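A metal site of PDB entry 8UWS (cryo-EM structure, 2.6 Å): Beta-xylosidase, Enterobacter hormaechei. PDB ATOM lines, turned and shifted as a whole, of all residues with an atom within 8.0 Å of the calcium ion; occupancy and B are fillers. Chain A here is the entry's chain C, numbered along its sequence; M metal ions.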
ATOM      1  N   ARG A 332      10.940 -15.351 -28.059  1.00  0.00           N
ATOM      2  CA  ARG A 332      10.723 -16.539 -27.237  1.00  0.00           C
ATOM      3  C   ARG A 332      10.646 -17.762 -28.130  1.00  0.00           C
ATOM      4  O   ARG A 332      10.249 -17.674 -29.288  1.00  0.00           O
ATOM      5  CB  ARG A 332       9.449 -16.412 -26.395  1.00  0.00           C
ATOM      6  CG  ARG A 332       8.166 -16.580 -27.177  1.00  0.00           C
ATOM      7  CD  ARG A 332       7.182 -17.442 -26.408  1.00  0.00           C
ATOM      8  NE  ARG A 332       7.097 -17.047 -25.013  1.00  0.00           N
ATOM      9  CZ  ARG A 332       6.325 -17.640 -24.111  1.00  0.00           C
ATOM     10  NH1 ARG A 332       5.554 -18.665 -24.426  1.00  0.00           N
ATOM     11  NH2 ARG A 332       6.333 -17.201 -22.859  1.00  0.00           N
ATOM     12  N   ASP A 333      11.032 -18.910 -27.570  1.00  0.00           N
ATOM     13  CA  ASP A 333      10.948 -20.205 -28.249  1.00  0.00           C
ATOM     14  C   ASP A 333      10.272 -21.187 -27.322  1.00  0.00           C
ATOM     15  O   ASP A 333      10.801 -21.496 -26.251  1.00  0.00           O
ATOM     16  CB  ASP A 333      12.343 -20.697 -28.652  1.00  0.00           C
ATOM     17  CG  ASP A 333      12.287 -21.700 -29.787  1.00  0.00           C
ATOM     18  OD1 ASP A 333      13.273 -22.443 -29.970  1.00  0.00           O
ATOM     19  OD2 ASP A 333      11.274 -21.737 -30.499  1.00  0.00           O
ATOM     20  N   ASP A 334       9.107 -21.690 -27.728  1.00  0.00           N
ATOM     21  CA  ASP A 334       8.360 -22.652 -26.923  1.00  0.00           C
ATOM     22  C   ASP A 334       8.716 -24.098 -27.234  1.00  0.00           C
ATOM     23  O   ASP A 334       8.140 -25.007 -26.617  1.00  0.00           O
ATOM     24  CB  ASP A 334       6.863 -22.427 -27.102  1.00  0.00           C
ATOM     25  CG  ASP A 334       6.381 -21.124 -26.517  1.00  0.00           C
ATOM     26  OD1 ASP A 334       6.424 -20.977 -25.274  1.00  0.00           O
ATOM     27  OD2 ASP A 334       5.954 -20.241 -27.295  1.00  0.00           O
ATOM     28  N   PHE A 335       9.638 -24.330 -28.170  1.00  0.00           N
ATOM     29  CA  PHE A 335      10.137 -25.664 -28.487  1.00  0.00           C
ATOM     30  C   PHE A 335       9.023 -26.617 -28.917  1.00  0.00           C
ATOM     31  O   PHE A 335       8.916 -27.732 -28.411  1.00  0.00           O
ATOM     32  CB  PHE A 335      10.922 -26.253 -27.307  1.00  0.00           C
ATOM     33  CG  PHE A 335      12.096 -25.438 -26.877  1.00  0.00           C
ATOM     34  CD1 PHE A 335      13.015 -24.975 -27.813  1.00  0.00           C
ATOM     35  CD2 PHE A 335      12.305 -25.147 -25.544  1.00  0.00           C
ATOM     36  CE1 PHE A 335      14.100 -24.233 -27.408  1.00  0.00           C
ATOM     37  CE2 PHE A 335      13.388 -24.397 -25.145  1.00  0.00           C
ATOM     38  CZ  PHE A 335      14.285 -23.940 -26.077  1.00  0.00           C
ATOM     39  N   ASP A 336       8.200 -26.183 -29.868  1.00  0.00           N
ATOM     40  CA  ASP A 336       7.137 -27.047 -30.382  1.00  0.00           C
ATOM     41  C   ASP A 336       7.487 -27.685 -31.714  1.00  0.00           C
ATOM     42  O   ASP A 336       6.913 -28.738 -32.046  1.00  0.00           O
ATOM     43  CB  ASP A 336       5.838 -26.253 -30.538  1.00  0.00           C
ATOM     44  CG  ASP A 336       5.621 -25.253 -29.433  1.00  0.00           C
ATOM     45  OD1 ASP A 336       4.830 -25.540 -28.515  1.00  0.00           O
ATOM     46  OD2 ASP A 336       6.227 -24.165 -29.503  1.00  0.00           O
ATOM     47  N   GLY A 337       8.381 -27.087 -32.489  1.00  0.00           N
ATOM     48  CA  GLY A 337       8.665 -27.573 -33.833  1.00  0.00           C
ATOM     49  C   GLY A 337       9.715 -28.661 -33.888  1.00  0.00           C
ATOM     50  O   GLY A 337       9.921 -29.388 -32.909  1.00  0.00           O
ATOM     51  N   ARG A 361      10.441 -35.766 -26.143  1.00  0.00           N
ATOM     52  CA  ARG A 361       9.285 -35.270 -25.396  1.00  0.00           C
ATOM     53  C   ARG A 361       8.770 -34.042 -26.123  1.00  0.00           C
ATOM     54  O   ARG A 361       9.376 -32.962 -26.054  1.00  0.00           O
ATOM     55  CB  ARG A 361       9.655 -34.940 -23.950  1.00  0.00           C
ATOM     56  CG  ARG A 361       8.525 -34.333 -23.131  1.00  0.00           C
ATOM     57  CD  ARG A 361       8.803 -34.494 -21.653  1.00  0.00           C
ATOM     58  NE  ARG A 361       7.691 -34.037 -20.826  1.00  0.00           N
ATOM     59  CZ  ARG A 361       7.832 -33.507 -19.615  1.00  0.00           C
ATOM     60  NH1 ARG A 361       9.018 -33.360 -19.056  1.00  0.00           N
ATOM     61  NH2 ARG A 361       6.746 -33.122 -18.954  1.00  0.00           N
ATOM     62  N   PRO A 362       7.670 -34.172 -26.854  1.00  0.00           N
ATOM     63  CA  PRO A 362       7.170 -33.044 -27.644  1.00  0.00           C
ATOM     64  C   PRO A 362       6.844 -31.852 -26.762  1.00  0.00           C
ATOM     65  O   PRO A 362       6.295 -31.985 -25.667  1.00  0.00           O
ATOM     66  CB  PRO A 362       5.905 -33.604 -28.314  1.00  0.00           C
ATOM     67  CG  PRO A 362       6.105 -35.076 -28.314  1.00  0.00           C
ATOM     68  CD  PRO A 362       6.861 -35.380 -27.056  1.00  0.00           C
ATOM     69  N   GLY A 363       7.189 -30.660 -27.248  1.00  0.00           N
ATOM     70  CA  GLY A 363       6.972 -29.438 -26.519  1.00  0.00           C
ATOM     71  C   GLY A 363       8.073 -29.061 -25.556  1.00  0.00           C
ATOM     72  O   GLY A 363       8.001 -27.983 -24.943  1.00  0.00           O
ATOM     73  N   TYR A 364       9.093 -29.900 -25.394  1.00  0.00           N
ATOM     74  CA  TYR A 364      10.191 -29.622 -24.484  1.00  0.00           C
ATOM     75  C   TYR A 364      11.525 -29.846 -25.176  1.00  0.00           C
ATOM     76  O   TYR A 364      11.635 -30.699 -26.065  1.00  0.00           O
ATOM     77  CB  TYR A 364      10.117 -30.517 -23.233  1.00  0.00           C
ATOM     78  CG  TYR A 364       8.961 -30.214 -22.306  1.00  0.00           C
ATOM     79  CD1 TYR A 364       7.675 -30.632 -22.612  1.00  0.00           C
ATOM     80  CD2 TYR A 364       9.155 -29.531 -21.119  1.00  0.00           C
ATOM     81  CE1 TYR A 364       6.619 -30.370 -21.769  1.00  0.00           C
ATOM     82  CE2 TYR A 364       8.103 -29.262 -20.270  1.00  0.00           C
ATOM     83  CZ  TYR A 364       6.838 -29.689 -20.597  1.00  0.00           C
ATOM     84  OH  TYR A 364       5.794 -29.421 -19.753  1.00  0.00           O
ATOM     85  N   LEU A 365      12.528 -29.085 -24.755  1.00  0.00           N
ATOM     86  CA  LEU A 365      13.896 -29.255 -25.235  1.00  0.00           C
ATOM     87  C   LEU A 365      14.645 -30.124 -24.227  1.00  0.00           C
ATOM     88  O   LEU A 365      14.980 -29.663 -23.132  1.00  0.00           O
ATOM     89  CB  LEU A 365      14.591 -27.910 -25.419  1.00  0.00           C
ATOM     90  CG  LEU A 365      16.108 -27.951 -25.620  1.00  0.00           C
ATOM     91  CD1 LEU A 365      16.469 -28.512 -26.963  1.00  0.00           C
ATOM     92  CD2 LEU A 365      16.701 -26.559 -25.448  1.00  0.00           C
ATOM     93  N   PHE A 528      13.508 -28.405 -20.789  1.00  0.00           N
ATOM     94  CA  PHE A 528      13.229 -26.977 -20.720  1.00  0.00           C
ATOM     95  C   PHE A 528      11.997 -26.694 -21.561  1.00  0.00           C
ATOM     96  O   PHE A 528      11.952 -27.039 -22.746  1.00  0.00           O
ATOM     97  CB  PHE A 528      14.422 -26.165 -21.227  1.00  0.00           C
ATOM     98  CG  PHE A 528      15.683 -26.414 -20.459  1.00  0.00           C
ATOM     99  CD1 PHE A 528      16.603 -27.350 -20.891  1.00  0.00           C
ATOM    100  CD2 PHE A 528      15.957 -25.694 -19.317  1.00  0.00           C
ATOM    101  CE1 PHE A 528      17.760 -27.570 -20.184  1.00  0.00           C
ATOM    102  CE2 PHE A 528      17.114 -25.915 -18.610  1.00  0.00           C
ATOM    103  CZ  PHE A 528      18.022 -26.857 -19.043  1.00  0.00           C
ATOM    104  N   ASP A 529      10.991 -26.080 -20.945  1.00  0.00           N
ATOM    105  CA  ASP A 529       9.739 -25.811 -21.660  1.00  0.00           C
ATOM    106  C   ASP A 529       9.898 -24.696 -22.672  1.00  0.00           C
ATOM    107  O   ASP A 529       9.471 -24.818 -23.821  1.00  0.00           O
ATOM    108  CB  ASP A 529       8.625 -25.489 -20.665  1.00  0.00           C
ATOM    109  CG  ASP A 529       7.249 -25.510 -21.304  1.00  0.00           C
ATOM    110  OD1 ASP A 529       6.260 -25.251 -20.583  1.00  0.00           O
ATOM    111  OD2 ASP A 529       7.157 -25.788 -22.517  1.00  0.00           O
ATOM    112  N   TYR A 530      10.524 -23.583 -22.277  1.00  0.00           N
ATOM    113  CA  TYR A 530      10.599 -22.421 -23.140  1.00  0.00           C
ATOM    114  C   TYR A 530      11.835 -21.589 -22.785  1.00  0.00           C
ATOM    115  O   TYR A 530      12.509 -21.844 -21.789  1.00  0.00           O
ATOM    116  CB  TYR A 530       9.309 -21.587 -23.070  1.00  0.00           C
ATOM    117  CG  TYR A 530       8.895 -21.100 -21.691  1.00  0.00           C
ATOM    118  CD1 TYR A 530       9.766 -20.431 -20.852  1.00  0.00           C
ATOM    119  CD2 TYR A 530       7.603 -21.303 -21.239  1.00  0.00           C
ATOM    120  CE1 TYR A 530       9.374 -19.981 -19.611  1.00  0.00           C
ATOM    121  CE2 TYR A 530       7.202 -20.865 -19.993  1.00  0.00           C
ATOM    122  CZ  TYR A 530       8.088 -20.204 -19.187  1.00  0.00           C
ATOM    123  OH  TYR A 530       7.694 -19.768 -17.946  1.00  0.00           O
ATOM    124  N   PHE A 531      12.106 -20.603 -23.631  1.00  0.00           N
ATOM    125  CA  PHE A 531      13.196 -19.661 -23.417  1.00  0.00           C
ATOM    126  C   PHE A 531      12.736 -18.297 -23.908  1.00  0.00           C
ATOM    127  O   PHE A 531      12.441 -18.136 -25.098  1.00  0.00           O
ATOM    128  CB  PHE A 531      14.454 -20.107 -24.156  1.00  0.00           C
ATOM    129  CG  PHE A 531      15.709 -19.433 -23.672  1.00  0.00           C
ATOM    130  CD1 PHE A 531      15.785 -18.927 -22.391  1.00  0.00           C
ATOM    131  CD2 PHE A 531      16.794 -19.307 -24.507  1.00  0.00           C
ATOM    132  CE1 PHE A 531      16.938 -18.310 -21.957  1.00  0.00           C
ATOM    133  CE2 PHE A 531      17.947 -18.689 -24.073  1.00  0.00           C
ATOM    134  CZ  PHE A 531      18.010 -18.190 -22.793  1.00  0.00           C
HETATM  135 CA    CA M   1       6.466 -26.056 -24.928  1.00  0.00          CA
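OD1 of Asp 334 lies within salt-bridge range of NH1 of Arg 332.
Asp 336 touches the calcium ion (OD1 to CA, 3.98 Å). Within 4 Å of the calcium ion: Asp 334, Asp 336, Gly 363 and Asp 529. The nearest printed residue that does not touch the calcium ion is Phe 335 (4.6 Å).
O of Gly 363 is bound to the calcium ion (2.5 Å). OD2 of Asp 529 is bound to the calcium ion (2.5 Å). O of Asp 334 is bound to the calcium ion, 2.6 Å away.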
